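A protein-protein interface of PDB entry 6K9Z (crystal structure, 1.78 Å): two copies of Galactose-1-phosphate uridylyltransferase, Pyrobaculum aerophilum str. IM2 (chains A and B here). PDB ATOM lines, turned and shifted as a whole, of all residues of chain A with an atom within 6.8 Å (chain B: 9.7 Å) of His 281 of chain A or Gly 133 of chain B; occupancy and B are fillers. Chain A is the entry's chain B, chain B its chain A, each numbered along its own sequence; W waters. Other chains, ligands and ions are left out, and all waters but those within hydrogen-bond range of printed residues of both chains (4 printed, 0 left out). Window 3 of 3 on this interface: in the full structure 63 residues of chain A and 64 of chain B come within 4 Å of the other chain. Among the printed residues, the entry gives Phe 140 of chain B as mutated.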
ATOM      1  N   GLU A 131      21.756   8.979  -2.285  1.00  0.00           N
ATOM      2  CA  GLU A 131      21.456   7.578  -1.795  1.00  0.00           C
ATOM      3  C   GLU A 131      22.737   6.775  -1.556  1.00  0.00           C
ATOM      4  O   GLU A 131      22.644   5.745  -0.889  1.00  0.00           O
ATOM      5  CB  GLU A 131      20.534   6.866  -2.777  1.00  0.00           C
ATOM      6  CG  GLU A 131      19.127   7.390  -2.660  1.00  0.00           C
ATOM      7  CD  GLU A 131      18.261   6.823  -3.758  1.00  0.00           C
ATOM      8  OE1 GLU A 131      18.496   7.240  -4.880  1.00  0.00           O
ATOM      9  OE2 GLU A 131      17.517   5.844  -3.489  1.00  0.00           O
ATOM     10  N   TRP A 200      27.183  -5.087 -11.076  1.00  0.00           N
ATOM     11  CA  TRP A 200      26.254  -4.072 -10.525  1.00  0.00           C
ATOM     12  C   TRP A 200      25.067  -3.929 -11.455  1.00  0.00           C
ATOM     13  O   TRP A 200      25.131  -4.384 -12.607  1.00  0.00           O
ATOM     14  CB  TRP A 200      27.007  -2.781 -10.253  1.00  0.00           C
ATOM     15  CG  TRP A 200      28.154  -2.991  -9.319  1.00  0.00           C
ATOM     16  CD1 TRP A 200      29.478  -3.052  -9.645  1.00  0.00           C
ATOM     17  CD2 TRP A 200      28.059  -3.298  -7.929  1.00  0.00           C
ATOM     18  NE1 TRP A 200      30.204  -3.424  -8.541  1.00  0.00           N
ATOM     19  CE2 TRP A 200      29.369  -3.508  -7.467  1.00  0.00           C
ATOM     20  CE3 TRP A 200      26.995  -3.418  -7.035  1.00  0.00           C
ATOM     21  CZ2 TRP A 200      29.632  -3.866  -6.148  1.00  0.00           C
ATOM     22  CZ3 TRP A 200      27.262  -3.746  -5.719  1.00  0.00           C
ATOM     23  CH2 TRP A 200      28.566  -3.975  -5.290  1.00  0.00           C
ATOM     24  N   MET A 272      23.562   2.077  -9.667  1.00  0.00           N
ATOM     25  CA  MET A 272      23.191   1.372  -8.433  1.00  0.00           C
ATOM     26  C   MET A 272      21.674   1.263  -8.278  1.00  0.00           C
ATOM     27  O   MET A 272      21.204   0.781  -7.232  1.00  0.00           O
ATOM     28  CB  MET A 272      23.837   2.058  -7.231  1.00  0.00           C
ATOM     29  CG  MET A 272      25.345   2.073  -7.284  1.00  0.00           C
ATOM     30  SD  MET A 272      26.061   0.362  -7.387  1.00  0.00           S
ATOM     31  CE  MET A 272      25.800  -0.116  -5.696  1.00  0.00           C
ATOM     32  N   ARG A 274      18.458  -1.047  -9.508  1.00  0.00           N
ATOM     33  CA  ARG A 274      17.880  -2.128 -10.333  1.00  0.00           C
ATOM     34  C   ARG A 274      16.935  -1.479 -11.367  1.00  0.00           C
ATOM     35  O   ARG A 274      16.424  -0.296 -11.211  1.00  0.00           O
ATOM     36  CB  ARG A 274      17.043  -3.102  -9.493  1.00  0.00           C
ATOM     37  CG  ARG A 274      17.843  -3.821  -8.420  1.00  0.00           C
ATOM     38  CD  ARG A 274      17.084  -5.021  -7.872  1.00  0.00           C
ATOM     39  NE  ARG A 274      17.813  -5.719  -6.809  1.00  0.00           N
ATOM     40  CZ  ARG A 274      18.029  -5.226  -5.580  1.00  0.00           C
ATOM     41  NH1 ARG A 274      17.597  -4.013  -5.256  1.00  0.00           N
ATOM     42  NH2 ARG A 274      18.703  -5.937  -4.686  1.00  0.00           N
ATOM     43  N   LEU A 279      17.208   1.009  -5.006  1.00  0.00           N
ATOM     44  CA  LEU A 279      18.662   1.061  -4.747  1.00  0.00           C
ATOM     45  C   LEU A 279      19.175  -0.353  -4.451  1.00  0.00           C
ATOM     46  O   LEU A 279      18.541  -1.058  -3.630  1.00  0.00           O
ATOM     47  CB  LEU A 279      18.843   2.012  -3.565  1.00  0.00           C
ATOM     48  CG  LEU A 279      20.284   2.295  -3.156  1.00  0.00           C
ATOM     49  CD1 LEU A 279      21.099   2.868  -4.310  1.00  0.00           C
ATOM     50  CD2 LEU A 279      20.285   3.212  -1.941  1.00  0.00           C
ATOM     51  N   LYS A 280      20.252  -0.731  -5.073  1.00  0.00           N
ATOM     52  CA  LYS A 280      21.063  -1.938  -4.763  1.00  0.00           C
ATOM     53  C   LYS A 280      22.063  -1.552  -3.659  1.00  0.00           C
ATOM     54  O   LYS A 280      22.787  -0.581  -3.840  1.00  0.00           O
ATOM     55  CB  LYS A 280      21.793  -2.448  -5.997  1.00  0.00           C
ATOM     56  CG  LYS A 280      22.661  -3.689  -5.827  1.00  0.00           C
ATOM     57  CD  LYS A 280      21.893  -4.896  -5.329  1.00  0.00           C
ATOM     58  CE  LYS A 280      22.799  -6.096  -5.098  1.00  0.00           C
ATOM     59  NZ  LYS A 280      22.760  -7.017  -6.272  1.00  0.00           N
ATOM     60  N   HIS A 281      22.139  -2.304  -2.561  1.00  0.00           N
ATOM     61  CA  HIS A 281      23.123  -2.022  -1.470  1.00  0.00           C
ATOM     62  C   HIS A 281      24.210  -3.091  -1.533  1.00  0.00           C
ATOM     63  O   HIS A 281      23.856  -4.225  -1.775  1.00  0.00           O
ATOM     64  CB  HIS A 281      22.424  -1.984  -0.129  1.00  0.00           C
ATOM     65  CG  HIS A 281      21.503  -0.816   0.071  1.00  0.00           C
ATOM     66  ND1 HIS A 281      20.166  -0.845  -0.297  1.00  0.00           N
ATOM     67  CD2 HIS A 281      21.727   0.391   0.611  1.00  0.00           C
ATOM     68  CE1 HIS A 281      19.576   0.283   0.070  1.00  0.00           C
ATOM     69  NE2 HIS A 281      20.519   1.068   0.632  1.00  0.00           N
ATOM     70  N   ALA A 282      25.464  -2.717  -1.285  1.00  0.00           N
ATOM     71  CA  ALA A 282      26.518  -3.743  -1.159  1.00  0.00           C
ATOM     72  C   ALA A 282      26.429  -4.193   0.303  1.00  0.00           C
ATOM     73  O   ALA A 282      26.613  -3.336   1.183  1.00  0.00           O
ATOM     74  CB  ALA A 282      27.863  -3.144  -1.475  1.00  0.00           C
ATOM     75  N   ALA A 283      26.110  -5.465   0.549  1.00  0.00           N
ATOM     76  CA  ALA A 283      25.925  -5.931   1.943  1.00  0.00           C
ATOM     77  C   ALA A 283      26.727  -7.207   2.237  1.00  0.00           C
ATOM     78  O   ALA A 283      27.902  -7.266   1.860  1.00  0.00           O
ATOM     79  CB  ALA A 283      24.456  -6.085   2.248  1.00  0.00           C
ATOM     80  N   GLY A 284      26.094  -8.200   2.867  1.00  0.00           N
ATOM     81  CA  GLY A 284      26.821  -9.416   3.284  1.00  0.00           C
ATOM     82  C   GLY A 284      27.442 -10.209   2.146  1.00  0.00           C
ATOM     83  O   GLY A 284      28.624 -10.564   2.280  1.00  0.00           O
ATOM     84  N   GLU A 286      28.254  -9.107  -0.928  1.00  0.00           N
ATOM     85  CA  GLU A 286      29.258  -8.329  -1.671  1.00  0.00           C
ATOM     86  C   GLU A 286      30.432  -7.970  -0.750  1.00  0.00           C
ATOM     87  O   GLU A 286      31.553  -8.147  -1.171  1.00  0.00           O
ATOM     88  CB  GLU A 286      28.614  -7.041  -2.229  1.00  0.00           C
ATOM     89  CG  GLU A 286      27.447  -7.381  -3.184  1.00  0.00           C
ATOM     90  CD  GLU A 286      26.083  -7.636  -2.550  1.00  0.00           C
ATOM     91  OE1 GLU A 286      25.922  -7.562  -1.304  1.00  0.00           O
ATOM     92  OE2 GLU A 286      25.102  -7.877  -3.312  1.00  0.00           O
ATOM     93  N   LEU A 287      30.160  -7.365   0.372  1.00  0.00           N
ATOM     94  CA  LEU A 287      31.203  -6.831   1.289  1.00  0.00           C
ATOM     95  C   LEU A 287      31.789  -7.998   2.108  1.00  0.00           C
ATOM     96  O   LEU A 287      33.036  -7.999   2.330  1.00  0.00           O
ATOM     97  CB  LEU A 287      30.646  -5.791   2.230  1.00  0.00           C
ATOM     98  CG  LEU A 287      30.003  -4.578   1.545  1.00  0.00           C
ATOM     99  CD1 LEU A 287      29.600  -3.547   2.571  1.00  0.00           C
ATOM    100  CD2 LEU A 287      30.947  -4.013   0.502  1.00  0.00           C
ATOM    101  N   PHE B 125      25.213 -15.666   6.371  1.00  0.00           N
ATOM    102  CA  PHE B 125      25.347 -14.202   6.499  1.00  0.00           C
ATOM    103  C   PHE B 125      24.034 -13.609   6.972  1.00  0.00           C
ATOM    104  O   PHE B 125      23.006 -14.272   6.912  1.00  0.00           O
ATOM    105  CB  PHE B 125      25.859 -13.536   5.223  1.00  0.00           C
ATOM    106  CG  PHE B 125      24.953 -13.626   4.040  1.00  0.00           C
ATOM    107  CD1 PHE B 125      24.941 -14.767   3.256  1.00  0.00           C
ATOM    108  CD2 PHE B 125      24.090 -12.582   3.732  1.00  0.00           C
ATOM    109  CE1 PHE B 125      24.132 -14.835   2.134  1.00  0.00           C
ATOM    110  CE2 PHE B 125      23.251 -12.663   2.640  1.00  0.00           C
ATOM    111  CZ  PHE B 125      23.257 -13.789   1.838  1.00  0.00           C
ATOM    112  N   ASN B 127      22.029  -9.688   6.980  1.00  0.00           N
ATOM    113  CA  ASN B 127      21.941  -8.231   6.722  1.00  0.00           C
ATOM    114  C   ASN B 127      20.886  -7.659   7.663  1.00  0.00           C
ATOM    115  O   ASN B 127      19.810  -8.251   7.762  1.00  0.00           O
ATOM    116  CB  ASN B 127      21.562  -7.931   5.273  1.00  0.00           C
ATOM    117  CG  ASN B 127      22.603  -8.463   4.318  1.00  0.00           C
ATOM    118  OD1 ASN B 127      23.792  -8.216   4.530  1.00  0.00           O
ATOM    119  ND2 ASN B 127      22.153  -9.143   3.261  1.00  0.00           N
ATOM    120  N   LYS B 128      21.170  -6.498   8.295  1.00  0.00           N
ATOM    121  CA  LYS B 128      20.208  -5.944   9.272  1.00  0.00           C
ATOM    122  C   LYS B 128      20.090  -4.448   9.029  1.00  0.00           C
ATOM    123  O   LYS B 128      21.117  -3.765   9.016  1.00  0.00           O
ATOM    124  CB  LYS B 128      20.696  -6.239  10.698  1.00  0.00           C
ATOM    125  CG  LYS B 128      19.691  -5.882  11.775  1.00  0.00           C
ATOM    126  CD  LYS B 128      19.716  -4.434  12.245  1.00  0.00           C
ATOM    127  CE  LYS B 128      18.797  -4.214  13.431  1.00  0.00           C
ATOM    128  NZ  LYS B 128      19.101  -2.932  14.115  1.00  0.00           N
ATOM    129  N   GLY B 129      18.878  -3.979   8.786  1.00  0.00           N
ATOM    130  CA  GLY B 129      18.612  -2.542   8.698  1.00  0.00           C
ATOM    131  C   GLY B 129      17.997  -2.148   7.365  1.00  0.00           C
ATOM    132  O   GLY B 129      18.522  -2.492   6.295  1.00  0.00           O
ATOM    133  N   LYS B 130      16.927  -1.374   7.422  1.00  0.00           N
ATOM    134  CA  LYS B 130      16.307  -0.830   6.188  1.00  0.00           C
ATOM    135  C   LYS B 130      17.376  -0.028   5.398  1.00  0.00           C
ATOM    136  O   LYS B 130      17.331  -0.023   4.133  1.00  0.00           O
ATOM    137  CB  LYS B 130      15.100   0.031   6.573  1.00  0.00           C
ATOM    138  CG  LYS B 130      13.942  -0.785   7.129  1.00  0.00           C
ATOM    139  CD  LYS B 130      12.745   0.017   7.645  1.00  0.00           C
ATOM    140  CE  LYS B 130      11.762  -0.851   8.426  1.00  0.00           C
ATOM    141  NZ  LYS B 130      10.447  -0.179   8.586  1.00  0.00           N
ATOM    142  N   GLU B 131      18.292   0.638   6.103  1.00  0.00           N
ATOM    143  CA  GLU B 131      19.265   1.564   5.451  1.00  0.00           C
ATOM    144  C   GLU B 131      20.248   0.813   4.544  1.00  0.00           C
ATOM    145  O   GLU B 131      20.838   1.521   3.717  1.00  0.00           O
ATOM    146  CB  GLU B 131      20.022   2.402   6.485  1.00  0.00           C
ATOM    147  CG  GLU B 131      19.193   3.515   7.032  1.00  0.00           C
ATOM    148  CD  GLU B 131      19.823   4.211   8.219  1.00  0.00           C
ATOM    149  OE1 GLU B 131      19.848   3.590   9.254  1.00  0.00           O
ATOM    150  OE2 GLU B 131      20.290   5.374   8.064  1.00  0.00           O
ATOM    151  N   ILE B 132      20.379  -0.519   4.661  1.00  0.00           N
ATOM    152  CA  ILE B 132      21.263  -1.385   3.812  1.00  0.00           C
ATOM    153  C   ILE B 132      20.430  -2.394   3.007  1.00  0.00           C
ATOM    154  O   ILE B 132      20.995  -3.352   2.501  1.00  0.00           O
ATOM    155  CB  ILE B 132      22.412  -2.007   4.616  1.00  0.00           C
ATOM    156  CG1 ILE B 132      21.909  -3.014   5.652  1.00  0.00           C
ATOM    157  CG2 ILE B 132      23.284  -0.874   5.192  1.00  0.00           C
ATOM    158  CD1 ILE B 132      22.913  -4.067   5.998  1.00  0.00           C
ATOM    159  N   GLY B 133      19.147  -2.098   2.824  1.00  0.00           N
ATOM    160  CA  GLY B 133      18.295  -2.716   1.789  1.00  0.00           C
ATOM    161  C   GLY B 133      17.418  -3.818   2.349  1.00  0.00           C
ATOM    162  O   GLY B 133      16.761  -4.479   1.564  1.00  0.00           O
ATOM    163  N   VAL B 134      17.374  -4.003   3.672  1.00  0.00           N
ATOM    164  CA  VAL B 134      16.496  -5.045   4.266  1.00  0.00           C
ATOM    165  C   VAL B 134      15.098  -4.461   4.482  1.00  0.00           C
ATOM    166  O   VAL B 134      14.876  -3.815   5.546  1.00  0.00           O
ATOM    167  CB  VAL B 134      17.052  -5.634   5.566  1.00  0.00           C
ATOM    168  CG1 VAL B 134      16.223  -6.852   5.975  1.00  0.00           C
ATOM    169  CG2 VAL B 134      18.514  -5.978   5.386  1.00  0.00           C
ATOM    170  N   SER B 135      14.194  -4.781   3.577  1.00  0.00           N
ATOM    171  CA  SER B 135      12.790  -4.323   3.629  1.00  0.00           C
ATOM    172  C   SER B 135      11.957  -5.232   4.544  1.00  0.00           C
ATOM    173  O   SER B 135      11.156  -4.646   5.324  1.00  0.00           O
ATOM    174  CB  SER B 135      12.194  -4.166   2.238  1.00  0.00           C
ATOM    175  OG  SER B 135      12.525  -5.306   1.443  1.00  0.00           O
ATOM    176  N   LEU B 136      12.217  -6.565   4.562  1.00  0.00           N
ATOM    177  CA  LEU B 136      11.413  -7.486   5.417  1.00  0.00           C
ATOM    178  C   LEU B 136      11.844  -7.288   6.887  1.00  0.00           C
ATOM    179  O   LEU B 136      13.035  -7.348   7.166  1.00  0.00           O
ATOM    180  CB  LEU B 136      11.622  -8.935   4.964  1.00  0.00           C
ATOM    181  CG  LEU B 136      11.081  -9.316   3.589  1.00  0.00           C
ATOM    182  CD1 LEU B 136      11.651 -10.655   3.173  1.00  0.00           C
ATOM    183  CD2 LEU B 136       9.559  -9.371   3.553  1.00  0.00           C
ATOM    184  N   THR B 137      10.904  -7.116   7.814  1.00  0.00           N
ATOM    185  CA  THR B 137      11.188  -6.714   9.222  1.00  0.00           C
ATOM    186  C   THR B 137      11.325  -7.957  10.128  1.00  0.00           C
ATOM    187  O   THR B 137      11.913  -7.861  11.235  1.00  0.00           O
ATOM    188  CB  THR B 137      10.149  -5.680   9.667  1.00  0.00           C
ATOM    189  OG1 THR B 137       8.794  -6.097   9.418  1.00  0.00           O
ATOM    190  CG2 THR B 137      10.367  -4.374   8.925  1.00  0.00           C
ATOM    191  N   PHE B 140      15.709 -12.596  10.340  1.00  0.00           N
ATOM    192  CA  PHE B 140      16.166 -13.726   9.494  1.00  0.00           C
ATOM    193  C   PHE B 140      17.622 -13.496   9.096  1.00  0.00           C
ATOM    194  O   PHE B 140      18.126 -12.347   9.040  1.00  0.00           O
ATOM    195  CB  PHE B 140      15.288 -13.943   8.259  1.00  0.00           C
ATOM    196  CG  PHE B 140      15.506 -12.931   7.170  1.00  0.00           C
ATOM    197  CD1 PHE B 140      14.866 -11.709   7.223  1.00  0.00           C
ATOM    198  CD2 PHE B 140      16.366 -13.176   6.120  1.00  0.00           C
ATOM    199  CE1 PHE B 140      15.075 -10.755   6.243  1.00  0.00           C
ATOM    200  CE2 PHE B 140      16.586 -12.216   5.138  1.00  0.00           C
ATOM    201  CZ  PHE B 140      15.950 -11.007   5.210  1.00  0.00           C
ATOM    202  N   GLN B 142      20.609 -15.763   6.180  1.00  0.00           N
ATOM    203  CA  GLN B 142      20.634 -16.438   4.878  1.00  0.00           C
ATOM    204  C   GLN B 142      21.778 -17.445   4.884  1.00  0.00           C
ATOM    205  O   GLN B 142      22.812 -17.203   5.499  1.00  0.00           O
ATOM    206  CB  GLN B 142      20.748 -15.426   3.724  1.00  0.00           C
ATOM    207  CG  GLN B 142      19.505 -14.534   3.541  1.00  0.00           C
ATOM    208  CD  GLN B 142      19.566 -13.761   2.252  1.00  0.00           C
ATOM    209  OE1 GLN B 142      19.520 -14.309   1.127  1.00  0.00           O
ATOM    210  NE2 GLN B 142      19.663 -12.464   2.410  1.00  0.00           N
ATOM    211  N   PRO B 246      22.490  -0.301  11.532  1.00  0.00           N
ATOM    212  CA  PRO B 246      22.462  -1.346  10.515  1.00  0.00           C
ATOM    213  C   PRO B 246      23.817  -2.039  10.522  1.00  0.00           C
ATOM    214  O   PRO B 246      24.897  -1.418  10.732  1.00  0.00           O
ATOM    215  CB  PRO B 246      22.193  -0.609   9.201  1.00  0.00           C
ATOM    216  CG  PRO B 246      22.635   0.822   9.503  1.00  0.00           C
ATOM    217  CD  PRO B 246      22.412   1.052  10.979  1.00  0.00           C
ATOM    218  N   TYR B 247      23.801  -3.333  10.241  1.00  0.00           N
ATOM    219  CA  TYR B 247      25.074  -4.077  10.186  1.00  0.00           C
ATOM    220  C   TYR B 247      24.938  -5.272   9.245  1.00  0.00           C
ATOM    221  O   TYR B 247      23.799  -5.709   8.880  1.00  0.00           O
ATOM    222  CB  TYR B 247      25.518  -4.560  11.570  1.00  0.00           C
ATOM    223  CG  TYR B 247      24.624  -5.601  12.185  1.00  0.00           C
ATOM    224  CD1 TYR B 247      24.786  -6.929  11.861  1.00  0.00           C
ATOM    225  CD2 TYR B 247      23.619  -5.255  13.060  1.00  0.00           C
ATOM    226  CE1 TYR B 247      23.966  -7.915  12.378  1.00  0.00           C
ATOM    227  CE2 TYR B 247      22.784  -6.227  13.595  1.00  0.00           C
ATOM    228  CZ  TYR B 247      22.946  -7.546  13.227  1.00  0.00           C
ATOM    229  OH  TYR B 247      22.112  -8.518  13.692  1.00  0.00           O
ATOM    230  N   ILE B 248      26.121  -5.794   8.928  1.00  0.00           N
ATOM    231  CA  ILE B 248      26.339  -6.997   8.112  1.00  0.00           C
ATOM    232  C   ILE B 248      27.093  -7.961   9.004  1.00  0.00           C
ATOM    233  O   ILE B 248      28.040  -7.539   9.663  1.00  0.00           O
ATOM    234  CB  ILE B 248      27.134  -6.648   6.868  1.00  0.00           C
ATOM    235  CG1 ILE B 248      26.282  -5.762   5.956  1.00  0.00           C
ATOM    236  CG2 ILE B 248      27.649  -7.895   6.203  1.00  0.00           C
ATOM    237  CD1 ILE B 248      27.068  -4.750   5.198  1.00  0.00           C
ATOM    238  N   MET B 272      27.489  -0.213  10.313  1.00  0.00           N
ATOM    239  CA  MET B 272      27.631   0.674   9.130  1.00  0.00           C
ATOM    240  C   MET B 272      27.364   2.135   9.501  1.00  0.00           C
ATOM    241  O   MET B 272      27.332   2.959   8.605  1.00  0.00           O
ATOM    242  CB  MET B 272      26.775   0.199   7.954  1.00  0.00           C
ATOM    243  CG  MET B 272      27.171  -1.190   7.463  1.00  0.00           C
ATOM    244  SD  MET B 272      28.906  -1.158   6.872  1.00  0.00           S
ATOM    245  CE  MET B 272      28.648  -0.394   5.284  1.00  0.00           C
ATOM    246  N   LEU B 279      25.398   7.230   8.214  1.00  0.00           N
ATOM    247  CA  LEU B 279      25.459   5.930   7.500  1.00  0.00           C
ATOM    248  C   LEU B 279      26.669   5.937   6.558  1.00  0.00           C
ATOM    249  O   LEU B 279      26.898   6.959   5.895  1.00  0.00           O
ATOM    250  CB  LEU B 279      24.157   5.744   6.718  1.00  0.00           C
ATOM    251  CG  LEU B 279      24.053   4.456   5.906  1.00  0.00           C
ATOM    252  CD1 LEU B 279      24.214   3.237   6.799  1.00  0.00           C
ATOM    253  CD2 LEU B 279      22.730   4.395   5.158  1.00  0.00           C
ATOM    254  N   LYS B 280      27.393   4.819   6.492  1.00  0.00           N
ATOM    255  CA  LYS B 280      28.568   4.689   5.593  1.00  0.00           C
ATOM    256  C   LYS B 280      28.135   3.849   4.389  1.00  0.00           C
ATOM    257  O   LYS B 280      27.477   2.820   4.602  1.00  0.00           O
ATOM    258  CB  LYS B 280      29.743   4.028   6.322  1.00  0.00           C
ATOM    259  CG  LYS B 280      30.915   3.624   5.439  1.00  0.00           C
ATOM    260  CD  LYS B 280      31.796   4.788   5.045  1.00  0.00           C
ATOM    261  CE  LYS B 280      33.114   4.369   4.431  1.00  0.00           C
ATOM    262  NZ  LYS B 280      34.269   4.929   5.172  1.00  0.00           N
ATOM    263  N   HIS B 281      28.461   4.306   3.180  1.00  0.00           N
ATOM    264  CA  HIS B 281      28.083   3.579   1.941  1.00  0.00           C
ATOM    265  C   HIS B 281      29.341   3.094   1.220  1.00  0.00           C
ATOM    266  O   HIS B 281      30.289   3.880   1.113  1.00  0.00           O
ATOM    267  CB  HIS B 281      27.312   4.502   0.988  1.00  0.00           C
ATOM    268  CG  HIS B 281      25.956   4.902   1.460  1.00  0.00           C
ATOM    269  ND1 HIS B 281      25.740   6.051   2.186  1.00  0.00           N
ATOM    270  CD2 HIS B 281      24.746   4.332   1.287  1.00  0.00           C
ATOM    271  CE1 HIS B 281      24.457   6.165   2.454  1.00  0.00           C
ATOM    272  NE2 HIS B 281      23.827   5.122   1.915  1.00  0.00           N
ATOM    273  N   ALA B 282      29.361   1.836   0.784  1.00  0.00           N
ATOM    274  CA  ALA B 282      30.517   1.374  -0.010  1.00  0.00           C
ATOM    275  C   ALA B 282      30.373   2.083  -1.362  1.00  0.00           C
ATOM    276  O   ALA B 282      29.314   1.923  -1.991  1.00  0.00           O
ATOM    277  CB  ALA B 282      30.466  -0.122  -0.171  1.00  0.00           C
ATOM    278  N   ALA B 283      31.391   2.833  -1.792  1.00  0.00           N
ATOM    279  CA  ALA B 283      31.259   3.591  -3.059  1.00  0.00           C
ATOM    280  C   ALA B 283      32.483   3.418  -3.966  1.00  0.00           C
ATOM    281  O   ALA B 283      32.964   2.284  -4.112  1.00  0.00           O
ATOM    282  CB  ALA B 283      30.953   5.041  -2.780  1.00  0.00           C
ATOM    283  N   LEU B 287      34.164  -0.105  -3.674  1.00  0.00           N
ATOM    284  CA  LEU B 287      33.695  -1.041  -4.741  1.00  0.00           C
ATOM    285  C   LEU B 287      34.607  -0.938  -5.970  1.00  0.00           C
ATOM    286  O   LEU B 287      34.822  -1.975  -6.635  1.00  0.00           O
ATOM    287  CB  LEU B 287      32.233  -0.706  -5.070  1.00  0.00           C
ATOM    288  CG  LEU B 287      31.255  -0.773  -3.890  1.00  0.00           C
ATOM    289  CD1 LEU B 287      29.855  -0.515  -4.368  1.00  0.00           C
ATOM    290  CD2 LEU B 287      31.317  -2.104  -3.169  1.00  0.00           C
HETATM  291  O   HOH W   1      27.109  -0.308   1.433  1.00  0.00           O
HETATM  292  O   HOH W   2      26.618   0.100  -1.419  1.00  0.00           O
HETATM  293  O   HOH W   3      23.849  -9.746   0.800  1.00  0.00           O
HETATM  294  O   HOH W   4      33.245  -3.829  -8.988  1.00  0.00           O
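His 281 of chain A touches just these residues of chain B: Glu 131, Ile 132 and Gly 133.
Printed residues of chain A within 4 Å of Gly 133 of chain B: His 281 (3.4 Å).
No residue of chain B comes within 4 Å of Lys 280 of chain A.
Of the printed residues of chain B, Gly 284 of chain A touches Asn 127 and Ile 248.
Of the printed residues of chain A, Glu 131 of chain B touches His 281 (3.1 Å).
Of the printed residues of chain A, His 281 of chain B touches Glu 131 (3.1 Å).
Of the printed residues of chain B, Ala 282 of chain A touches Leu 287.
Printed residues of chain B within 4 Å of Glu 131 of chain A: His 281 (3.1 Å).
Ser 135 of chain B touches none of the printed residues of chain A.
Gln 142 of chain B touches none of the printed residues of chain A.
The nearest residue of chain B that does not touch His 281 of chain A is Lys 130 of chain B (4.7 Å).
The nearest residue of chain A that does not touch Gly 133 of chain B is Leu 279 of chain A (5.7 Å).
The nearest printed residue of chain A that does not touch His 281 of chain B is His 281 of chain A (5.0 Å).
The backbone NH (N) of Ala 283 of chain A sits at hydrogen-bond distance from the side-chain carboxylate (OE1) of Glu 286 of chain A.
Among the printed residues, pairs that only touch across the chains: Ala 283 of chain A with Asn 127 of chain B (3.2 Å), His 281 of chain A with Ile 132 of chain B (3.3 Å), His 281 of chain A with Gly 133 of chain B (3.4 Å), Gly 284 of chain A with Ile 248 of chain B (3.4 Å), Ala 283 of chain A with Ile 248 of chain B (3.6 Å), Trp 200 of chain A with Leu 287 of chain B (3.8 Å), Leu 287 of chain A with Ile 248 of chain B (3.8 Å), Leu 287 of chain A with Ala 282 of chain B (3.98 Å) and Ala 282 of chain A with Leu 287 of chain B (3.99 Å).
Water W2 lies within hydrogen-bond range of the backbone NH of Ala 282 of chain A (3.0 Å) and the backbone carbonyl oxygen of Ala 282 of chain B (3.3 Å).
Water W3 bridges ND2 of Asn 127 of chain B (3.0 Å) and N of Gly 284 of chain A (3.4 Å).
Water W1 bridges O of Ala 282 of chain A and N of Ala 282 of chain B.
Water W4 lies within hydrogen-bond range of NE1 of Trp 200 of chain A (3.1 Å) and O of Leu 287 of chain B (3.4 Å).
Of the 12 printed residues of chain A, 7 touch a printed residue of chain B.
Hydrophobic or aromatic side chains of chain A within 4 Å of the printed part of chain B: Trp 200, His 281, Ala 282, Ala 283 and Leu 287.
Hydrophobic or aromatic side chains of chain B within 4 Å of the printed part of chain A: Ile 248, His 281, Ala 282 and Leu 287.
Among the printed residues, 12 pairs touch across the chains.
Glu 131 of chain A touches His 281 of chain B, and with the chains exchanged His 281 of chain A touches Glu 131 of chain B.
Ala 282 of chain A touches Leu 287 of chain B, and with the chains exchanged Leu 287 of chain A touches Ala 282 of chain B.
Of the 12 pairs that touch across the chains among the printed residues, 4 have their exchanged pair printed and touching as well.
OD1 of Asn 127 of chain B is in hydrogen-bond range of N of Gly 284 of chain A (2.8 Å).
The backbone carbonyl oxygen (O) of Glu 131 of chain B lies within hydrogen-bond range of a ring nitrogen (NE2) of His 281 of chain A (3.1 Å).
A ring nitrogen (NE2) of His 281 of chain B sits at hydrogen-bond distance from the backbone carbonyl oxygen of Glu 131 of chain A.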
